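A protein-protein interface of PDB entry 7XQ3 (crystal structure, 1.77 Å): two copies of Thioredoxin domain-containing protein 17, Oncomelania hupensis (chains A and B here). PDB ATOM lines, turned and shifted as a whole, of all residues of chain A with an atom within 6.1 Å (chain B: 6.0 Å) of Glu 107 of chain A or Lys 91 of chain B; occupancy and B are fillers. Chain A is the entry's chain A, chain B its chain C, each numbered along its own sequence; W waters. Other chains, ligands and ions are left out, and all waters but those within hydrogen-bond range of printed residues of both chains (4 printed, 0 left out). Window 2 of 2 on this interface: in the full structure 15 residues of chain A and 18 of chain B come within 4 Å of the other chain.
Water W2 bridges OE1 of Glu 106 of chain A (2.5 Å) and OE2 of Glu 106 of chain B (3.1 Å). Water W4 bridges the side-chain amide oxygen (OE1) of Gln 109 of chain A (2.7 Å) and the guanidinium group (NH2) of Arg 104 of chain B (3.4 Å). Water W1 lies within hydrogen-bond range of the side-chain carboxylate (OE1) of Glu 106 of chain A, the side-chain carboxylate (OE1) of Glu 106 of chain B and the side-chain amino group (NZ) of Lys 91 of chain B. Water W3 bridges OE1 of Glu 106 of chain B (2.8 Å) and OE2 of Glu 106 of chain A (3.0 Å).
CG of Lys 89 of chain B touches NE2 of Gln 109 of chain A (3.8 Å). Gln 109 of chain A touches Arg 104 of chain B.
The side-chain amino group (NZ) of Lys 91 of chain A lies within hydrogen-bond range of the side-chain sulfur (SG) of Cys 92 of chain B (3.4 Å). NZ of Lys 91 of chain A is in salt-bridge range of OE1 of Glu 106 of chain B (2.9 Å). The side-chain sulfur (SG) of Cys 92 of chain A sits at hydrogen-bond distance from the side-chain amino group (NZ) of Lys 91 of chain B, 3.2 Å away. OE1 of Glu 106 of chain A lies within salt-bridge range of NZ of Lys 91 of chain B (2.8 Å). The side-chain carboxylate (OE1) of Glu 107 of chain A is in salt-bridge range of the side-chain amino group (NZ) of Lys 91 of chain B, 3.3 Å away.
Of chain B, only Lys 91 comes within 4 Å of Glu 107 of chain A. Lys 91 of chain B touches just these residues of chain A: Cys 92 (3.2 Å), Glu 106 (2.8 Å) and Glu 107 (3.3 Å). Printed residues of chain B within 4 Å of Glu 106 of chain A: Lys 91. Printed residues of chain B within 4 Å of Lys 91 of chain A: Cys 92 and Glu 106. Printed residues of chain A within 4 Å of Cys 92 of chain B: Lys 91. Of the printed residues of chain A, Arg 104 of chain B touches Gln 109. Pro 94 of chain A touches none of the printed residues of chain B. Glu 108 of chain A touches none of the printed residues of chain B. The nearest residue of chain A that does not touch Lys 91 of chain B is Lys 91 of chain A (4.7 Å). The nearest printed residue of chain B that does not touch Glu 106 of chain A is Glu 106 of chain B (4.6 Å).
The backbone carbonyl oxygen (O) of Cys 92 of chain A sits at hydrogen-bond distance from the side-chain hydroxyl (OG1) of Thr 95 of chain A, 2.7 Å away. SG of Cys 92 of chain A lies close to OE1 of Glu 106 of chain A (3.6 Å). The backbone carbonyl oxygen of Pro 94 of chain A is in hydrogen-bond range of the backbone NH of Glu 107 of chain A (3.0 Å). O of Lys 89 of chain B lies within hydrogen-bond range of NH1 of Arg 104 of chain B (3.4 Å). The side-chain hydroxyl (OG1) of Thr 95 of chain B is in hydrogen-bond range of the backbone carbonyl oxygen (O) of Cys 92 of chain B, at 2.7 Å. The side-chain sulfur of Cys 92 of chain B sits close to the side-chain carboxylate of Glu 106 of chain B (3.7 Å).
Of the 11 printed residues of chain B, 5 touch a printed residue of chain A. Among the printed residues, 7 pairs touch across the chains. Among the printed residues, Asp or Glu carboxylates within 4 Å of a Lys or Arg side-chain nitrogen of the other chain: Lys 91 of chain A with Glu 106 of chain B (2.9 Å), Glu 106 of chain A with Lys 91 of chain B (2.8 Å) and Glu 107 of chain A with Lys 91 of chain B (3.3 Å).
Lys 91 of chain A touches Cys 92 of chain B, and with the chains exchanged Cys 92 of chain A touches Lys 91 of chain B. Lys 91 of chain A touches Glu 106 of chain B, and with the chains exchanged Glu 106 of chain A touches Lys 91 of chain B. 5 positions are printed for both chains.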
ATOM      1  N   ASP A  43       1.330  42.707   0.663  1.00  0.00           N
ATOM      2  CA  ASP A  43       0.704  41.663   1.519  1.00  0.00           C
ATOM      3  C   ASP A  43       1.387  41.626   2.890  1.00  0.00           C
ATOM      4  O   ASP A  43       0.711  41.337   3.873  1.00  0.00           O
ATOM      5  CB  ASP A  43       0.723  40.284   0.866  1.00  0.00           C
ATOM      6  CG  ASP A  43      -0.362  40.045  -0.170  1.00  0.00           C
ATOM      7  OD1 ASP A  43      -1.370  40.782  -0.188  1.00  0.00           O
ATOM      8  OD2 ASP A  43      -0.175  39.119  -0.929  1.00  0.00           O
ATOM      9  N   ALA A  47      -0.427  42.234   6.548  1.00  0.00           N
ATOM     10  CA  ALA A  47      -0.314  41.158   7.565  1.00  0.00           C
ATOM     11  C   ALA A  47       0.184  41.705   8.915  1.00  0.00           C
ATOM     12  O   ALA A  47      -0.238  41.174   9.976  1.00  0.00           O
ATOM     13  CB  ALA A  47       0.579  40.070   7.006  1.00  0.00           C
ATOM     14  N   LYS A  91       8.439  30.165  -0.114  1.00  0.00           N
ATOM     15  CA  LYS A  91       7.928  30.253  -1.509  1.00  0.00           C
ATOM     16  C   LYS A  91       7.454  31.677  -1.802  1.00  0.00           C
ATOM     17  O   LYS A  91       7.160  32.002  -2.968  1.00  0.00           O
ATOM     18  CB  LYS A  91       6.845  29.187  -1.637  1.00  0.00           C
ATOM     19  CG  LYS A  91       7.438  27.787  -1.573  1.00  0.00           C
ATOM     20  CD  LYS A  91       6.441  26.708  -1.746  1.00  0.00           C
ATOM     21  CE  LYS A  91       6.733  25.799  -2.917  1.00  0.00           C
ATOM     22  NZ  LYS A  91       5.477  25.265  -3.492  1.00  0.00           N
ATOM     23  N   CYS A  92       7.299  32.498  -0.774  1.00  0.00           N
ATOM     24  CA  CYS A  92       6.740  33.865  -0.926  1.00  0.00           C
ATOM     25  C   CYS A  92       6.913  34.629   0.371  1.00  0.00           C
ATOM     26  O   CYS A  92       7.311  34.015   1.337  1.00  0.00           O
ATOM     27  CB  CYS A  92       5.268  33.816  -1.268  1.00  0.00           C
ATOM     28  SG  CYS A  92       4.368  32.888  -0.009  1.00  0.00           S
ATOM     29  N   VAL A  93       6.785  35.952   0.299  1.00  0.00           N
ATOM     30  CA  VAL A  93       6.607  36.838   1.474  1.00  0.00           C
ATOM     31  C   VAL A  93       5.252  37.508   1.316  1.00  0.00           C
ATOM     32  O   VAL A  93       4.829  37.882   0.210  1.00  0.00           O
ATOM     33  CB  VAL A  93       7.762  37.833   1.704  1.00  0.00           C
ATOM     34  CG1 VAL A  93       9.016  37.109   2.160  1.00  0.00           C
ATOM     35  CG2 VAL A  93       8.071  38.700   0.487  1.00  0.00           C
ATOM     36  N   PRO A  94       4.470  37.643   2.403  1.00  0.00           N
ATOM     37  CA  PRO A  94       4.851  37.186   3.735  1.00  0.00           C
ATOM     38  C   PRO A  94       4.647  35.678   3.903  1.00  0.00           C
ATOM     39  O   PRO A  94       3.776  35.082   3.249  1.00  0.00           O
ATOM     40  CB  PRO A  94       3.871  37.920   4.650  1.00  0.00           C
ATOM     41  CG  PRO A  94       2.639  38.084   3.784  1.00  0.00           C
ATOM     42  CD  PRO A  94       3.164  38.320   2.398  1.00  0.00           C
ATOM     43  N   THR A  95       5.516  35.073   4.720  1.00  0.00           N
ATOM     44  CA  THR A  95       5.293  33.719   5.261  1.00  0.00           C
ATOM     45  C   THR A  95       5.315  33.807   6.780  1.00  0.00           C
ATOM     46  O   THR A  95       6.260  34.321   7.308  1.00  0.00           O
ATOM     47  CB  THR A  95       6.283  32.683   4.726  1.00  0.00           C
ATOM     48  OG1 THR A  95       6.175  32.598   3.297  1.00  0.00           O
ATOM     49  CG2 THR A  95       6.068  31.306   5.331  1.00  0.00           C
ATOM     50  N   LEU A 105       1.497  29.828   7.008  1.00  0.00           N
ATOM     51  CA  LEU A 105       0.553  30.698   6.280  1.00  0.00           C
ATOM     52  C   LEU A 105       1.341  31.540   5.293  1.00  0.00           C
ATOM     53  O   LEU A 105       2.461  32.020   5.626  1.00  0.00           O
ATOM     54  CB  LEU A 105      -0.202  31.591   7.272  1.00  0.00           C
ATOM     55  CG  LEU A 105      -1.107  30.861   8.240  1.00  0.00           C
ATOM     56  CD1 LEU A 105      -1.745  31.826   9.269  1.00  0.00           C
ATOM     57  CD2 LEU A 105      -2.180  30.107   7.476  1.00  0.00           C
ATOM     58  N   GLU A 106       0.725  31.809   4.154  1.00  0.00           N
ATOM     59  CA  GLU A 106       1.392  32.600   3.097  1.00  0.00           C
ATOM     60  C   GLU A 106       0.465  33.655   2.519  1.00  0.00           C
ATOM     61  O   GLU A 106      -0.741  33.419   2.428  1.00  0.00           O
ATOM     62  CB  GLU A 106       1.814  31.693   1.950  1.00  0.00           C
ATOM     63  CG  GLU A 106       2.809  30.608   2.325  1.00  0.00           C
ATOM     64  CD  GLU A 106       3.365  29.811   1.144  1.00  0.00           C
ATOM     65  OE1 GLU A 106       2.648  29.680   0.100  1.00  0.00           O
ATOM     66  OE2 GLU A 106       4.510  29.311   1.264  1.00  0.00           O
ATOM     67  N   GLU A 107       1.061  34.759   2.102  1.00  0.00           N
ATOM     68  CA  GLU A 107       0.391  35.845   1.338  1.00  0.00           C
ATOM     69  C   GLU A 107      -0.833  36.333   2.113  1.00  0.00           C
ATOM     70  O   GLU A 107      -0.693  36.665   3.315  1.00  0.00           O
ATOM     71  CB  GLU A 107       0.109  35.360  -0.090  1.00  0.00           C
ATOM     72  CG  GLU A 107       1.394  35.082  -0.851  1.00  0.00           C
ATOM     73  CD  GLU A 107       1.262  34.745  -2.328  1.00  0.00           C
ATOM     74  OE1 GLU A 107       0.505  33.835  -2.663  1.00  0.00           O
ATOM     75  OE2 GLU A 107       1.973  35.383  -3.136  1.00  0.00           O
ATOM     76  N   GLU A 108      -2.022  36.344   1.501  1.00  0.00           N
ATOM     77  CA  GLU A 108      -3.208  36.959   2.153  1.00  0.00           C
ATOM     78  C   GLU A 108      -3.608  36.173   3.420  1.00  0.00           C
ATOM     79  O   GLU A 108      -4.285  36.756   4.287  1.00  0.00           O
ATOM     80  CB  GLU A 108      -4.347  37.042   1.141  1.00  0.00           C
ATOM     81  CG  GLU A 108      -3.936  37.718  -0.134  1.00  0.00           C
ATOM     82  CD  GLU A 108      -3.494  36.828  -1.290  1.00  0.00           C
ATOM     83  OE1 GLU A 108      -3.074  35.652  -1.057  1.00  0.00           O
ATOM     84  OE2 GLU A 108      -3.545  37.336  -2.440  1.00  0.00           O
ATOM     85  N   GLN A 109      -3.267  34.884   3.542  1.00  0.00           N
ATOM     86  CA  GLN A 109      -3.610  34.086   4.759  1.00  0.00           C
ATOM     87  C   GLN A 109      -2.913  34.673   5.994  1.00  0.00           C
ATOM     88  O   GLN A 109      -3.437  34.513   7.111  1.00  0.00           O
ATOM     89  CB  GLN A 109      -3.319  32.584   4.565  1.00  0.00           C
ATOM     90  CG  GLN A 109      -4.181  32.010   3.443  1.00  0.00           C
ATOM     91  CD  GLN A 109      -4.723  30.606   3.579  1.00  0.00           C
ATOM     92  OE1 GLN A 109      -3.999  29.664   3.900  1.00  0.00           O
ATOM     93  NE2 GLN A 109      -5.969  30.425   3.149  1.00  0.00           N
ATOM     94  N   CYS A 110      -1.790  35.370   5.821  1.00  0.00           N
ATOM     95  CA  CYS A 110      -1.070  36.067   6.929  1.00  0.00           C
ATOM     96  C   CYS A 110      -1.869  37.277   7.422  1.00  0.00           C
ATOM     97  O   CYS A 110      -1.550  37.741   8.521  1.00  0.00           O
ATOM     98  CB  CYS A 110       0.324  36.501   6.509  1.00  0.00           C
ATOM     99  SG  CYS A 110       1.365  35.085   6.122  1.00  0.00           S
ATOM    100  N   ALA A 111      -2.915  37.720   6.715  1.00  0.00           N
ATOM    101  CA  ALA A 111      -3.797  38.832   7.156  1.00  0.00           C
ATOM    102  C   ALA A 111      -5.194  38.301   7.489  1.00  0.00           C
ATOM    103  O   ALA A 111      -6.105  39.118   7.804  1.00  0.00           O
ATOM    104  CB  ALA A 111      -3.833  39.948   6.126  1.00  0.00           C
ATOM    105  N   TRP B  75      -4.097  22.122 -14.475  1.00  0.00           N
ATOM    106  CA  TRP B  75      -3.356  22.511 -13.257  1.00  0.00           C
ATOM    107  C   TRP B  75      -2.517  23.761 -13.557  1.00  0.00           C
ATOM    108  O   TRP B  75      -2.385  24.612 -12.661  1.00  0.00           O
ATOM    109  CB  TRP B  75      -2.507  21.360 -12.688  1.00  0.00           C
ATOM    110  CG  TRP B  75      -1.708  21.893 -11.552  1.00  0.00           C
ATOM    111  CD1 TRP B  75      -0.366  22.105 -11.493  1.00  0.00           C
ATOM    112  CD2 TRP B  75      -2.259  22.466 -10.354  1.00  0.00           C
ATOM    113  NE1 TRP B  75      -0.035  22.722 -10.318  1.00  0.00           N
ATOM    114  CE2 TRP B  75      -1.182  22.971  -9.609  1.00  0.00           C
ATOM    115  CE3 TRP B  75      -3.562  22.601  -9.851  1.00  0.00           C
ATOM    116  CZ2 TRP B  75      -1.362  23.589  -8.374  1.00  0.00           C
ATOM    117  CZ3 TRP B  75      -3.734  23.207  -8.627  1.00  0.00           C
ATOM    118  CH2 TRP B  75      -2.649  23.690  -7.903  1.00  0.00           C
ATOM    119  N   ARG B  83      -6.737  26.706  -7.285  1.00  0.00           N
ATOM    120  CA  ARG B  83      -5.789  27.817  -6.958  1.00  0.00           C
ATOM    121  C   ARG B  83      -6.543  29.029  -6.382  1.00  0.00           C
ATOM    122  O   ARG B  83      -5.964  29.733  -5.545  1.00  0.00           O
ATOM    123  CB  ARG B  83      -5.012  28.261  -8.195  1.00  0.00           C
ATOM    124  CG  ARG B  83      -4.147  27.181  -8.829  1.00  0.00           C
ATOM    125  CD  ARG B  83      -3.389  27.805  -9.985  1.00  0.00           C
ATOM    126  NE  ARG B  83      -2.486  26.864 -10.639  1.00  0.00           N
ATOM    127  CZ  ARG B  83      -1.213  26.675 -10.341  1.00  0.00           C
ATOM    128  NH1 ARG B  83      -0.647  27.314  -9.334  1.00  0.00           N
ATOM    129  NH2 ARG B  83      -0.510  25.797 -11.036  1.00  0.00           N
ATOM    130  N   LEU B  88      -8.727  26.500   0.094  1.00  0.00           N
ATOM    131  CA  LEU B  88      -7.610  25.620  -0.356  1.00  0.00           C
ATOM    132  C   LEU B  88      -6.392  26.461  -0.752  1.00  0.00           C
ATOM    133  O   LEU B  88      -5.285  26.135  -0.290  1.00  0.00           O
ATOM    134  CB  LEU B  88      -8.046  24.730  -1.512  1.00  0.00           C
ATOM    135  CG  LEU B  88      -9.194  23.774  -1.214  1.00  0.00           C
ATOM    136  CD1 LEU B  88      -9.442  22.888  -2.410  1.00  0.00           C
ATOM    137  CD2 LEU B  88      -8.914  22.897   0.008  1.00  0.00           C
ATOM    138  N   LYS B  89      -6.597  27.503  -1.565  1.00  0.00           N
ATOM    139  CA  LYS B  89      -5.523  28.398  -2.029  1.00  0.00           C
ATOM    140  C   LYS B  89      -4.326  27.561  -2.468  1.00  0.00           C
ATOM    141  O   LYS B  89      -3.216  27.877  -2.002  1.00  0.00           O
ATOM    142  CB  LYS B  89      -5.108  29.341  -0.890  1.00  0.00           C
ATOM    143  CG  LYS B  89      -5.984  30.565  -0.677  1.00  0.00           C
ATOM    144  CD  LYS B  89      -5.854  31.609  -1.774  1.00  0.00           C
ATOM    145  CE  LYS B  89      -6.185  33.022  -1.309  1.00  0.00           C
ATOM    146  NZ  LYS B  89      -7.641  33.203  -1.085  1.00  0.00           N
ATOM    147  N   LEU B  90      -4.525  26.527  -3.293  1.00  0.00           N
ATOM    148  CA  LEU B  90      -3.421  25.609  -3.687  1.00  0.00           C
ATOM    149  C   LEU B  90      -2.416  26.375  -4.537  1.00  0.00           C
ATOM    150  O   LEU B  90      -2.831  27.040  -5.471  1.00  0.00           O
ATOM    151  CB  LEU B  90      -3.935  24.438  -4.512  1.00  0.00           C
ATOM    152  CG  LEU B  90      -4.865  23.445  -3.836  1.00  0.00           C
ATOM    153  CD1 LEU B  90      -4.941  22.187  -4.710  1.00  0.00           C
ATOM    154  CD2 LEU B  90      -4.399  23.095  -2.429  1.00  0.00           C
ATOM    155  N   LYS B  91      -1.131  26.197  -4.273  1.00  0.00           N
ATOM    156  CA  LYS B  91      -0.049  26.847  -5.047  1.00  0.00           C
ATOM    157  C   LYS B  91       0.709  25.769  -5.814  1.00  0.00           C
ATOM    158  O   LYS B  91       1.452  26.093  -6.790  1.00  0.00           O
ATOM    159  CB  LYS B  91       0.800  27.665  -4.078  1.00  0.00           C
ATOM    160  CG  LYS B  91       0.009  28.846  -3.517  1.00  0.00           C
ATOM    161  CD  LYS B  91       0.751  29.705  -2.535  1.00  0.00           C
ATOM    162  CE  LYS B  91       1.721  30.670  -3.181  1.00  0.00           C
ATOM    163  NZ  LYS B  91       2.615  31.284  -2.168  1.00  0.00           N
ATOM    164  N   CYS B  92       0.520  24.506  -5.451  1.00  0.00           N
ATOM    165  CA  CYS B  92       1.264  23.444  -6.169  1.00  0.00           C
ATOM    166  C   CYS B  92       0.712  22.069  -5.847  1.00  0.00           C
ATOM    167  O   CYS B  92      -0.122  21.963  -4.952  1.00  0.00           O
ATOM    168  CB  CYS B  92       2.719  23.499  -5.758  1.00  0.00           C
ATOM    169  SG  CYS B  92       2.811  23.221  -3.988  1.00  0.00           S
ATOM    170  N   VAL B  93       1.122  21.076  -6.632  1.00  0.00           N
ATOM    171  CA  VAL B  93       0.859  19.648  -6.304  1.00  0.00           C
ATOM    172  C   VAL B  93       2.221  18.973  -6.245  1.00  0.00           C
ATOM    173  O   VAL B  93       3.133  19.350  -6.994  1.00  0.00           O
ATOM    174  CB  VAL B  93      -0.140  18.957  -7.255  1.00  0.00           C
ATOM    175  CG1 VAL B  93      -1.530  19.564  -7.123  1.00  0.00           C
ATOM    176  CG2 VAL B  93       0.317  18.959  -8.715  1.00  0.00           C
ATOM    177  N   THR B  95       0.107  18.897  -2.577  1.00  0.00           N
ATOM    178  CA  THR B  95      -0.185  19.628  -1.324  1.00  0.00           C
ATOM    179  C   THR B  95      -0.897  18.645  -0.401  1.00  0.00           C
ATOM    180  O   THR B  95      -1.858  18.015  -0.874  1.00  0.00           O
ATOM    181  CB  THR B  95      -1.045  20.893  -1.499  1.00  0.00           C
ATOM    182  OG1 THR B  95      -0.266  21.781  -2.293  1.00  0.00           O
ATOM    183  CG2 THR B  95      -1.357  21.559  -0.163  1.00  0.00           C
ATOM    184  N   ARG B 104      -0.121  22.684   6.500  1.00  0.00           N
ATOM    185  CA  ARG B 104       0.081  22.496   5.034  1.00  0.00           C
ATOM    186  C   ARG B 104       1.508  21.991   4.735  1.00  0.00           C
ATOM    187  O   ARG B 104       2.492  22.565   5.240  1.00  0.00           O
ATOM    188  CB  ARG B 104      -0.111  23.819   4.278  1.00  0.00           C
ATOM    189  CG  ARG B 104      -0.214  23.682   2.756  1.00  0.00           C
ATOM    190  CD  ARG B 104      -0.404  25.016   2.040  1.00  0.00           C
ATOM    191  NE  ARG B 104      -1.632  25.686   2.474  1.00  0.00           N
ATOM    192  CZ  ARG B 104      -2.704  25.890   1.723  1.00  0.00           C
ATOM    193  NH1 ARG B 104      -2.748  25.516   0.451  1.00  0.00           N
ATOM    194  NH2 ARG B 104      -3.765  26.436   2.279  1.00  0.00           N
ATOM    195  N   GLU B 106       3.987  20.941   1.138  1.00  0.00           N
ATOM    196  CA  GLU B 106       4.002  21.129  -0.331  1.00  0.00           C
ATOM    197  C   GLU B 106       5.214  20.412  -0.933  1.00  0.00           C
ATOM    198  O   GLU B 106       6.268  20.352  -0.273  1.00  0.00           O
ATOM    199  CB  GLU B 106       4.008  22.611  -0.687  1.00  0.00           C
ATOM    200  CG  GLU B 106       2.690  23.363  -0.431  1.00  0.00           C
ATOM    201  CD  GLU B 106       2.665  24.818  -0.910  1.00  0.00           C
ATOM    202  OE1 GLU B 106       3.771  25.390  -1.200  1.00  0.00           O
ATOM    203  OE2 GLU B 106       1.553  25.383  -0.988  1.00  0.00           O
HETATM  204  O   HOH W   1       3.613  28.097  -1.901  1.00  0.00           O
HETATM  205  O   HOH W   2       0.804  27.991   0.461  1.00  0.00           O
HETATM  206  O   HOH W   3       4.918  26.356   1.141  1.00  0.00           O
HETATM  207  O   HOH W   4      -4.984  27.530   5.208  1.00  0.00           O
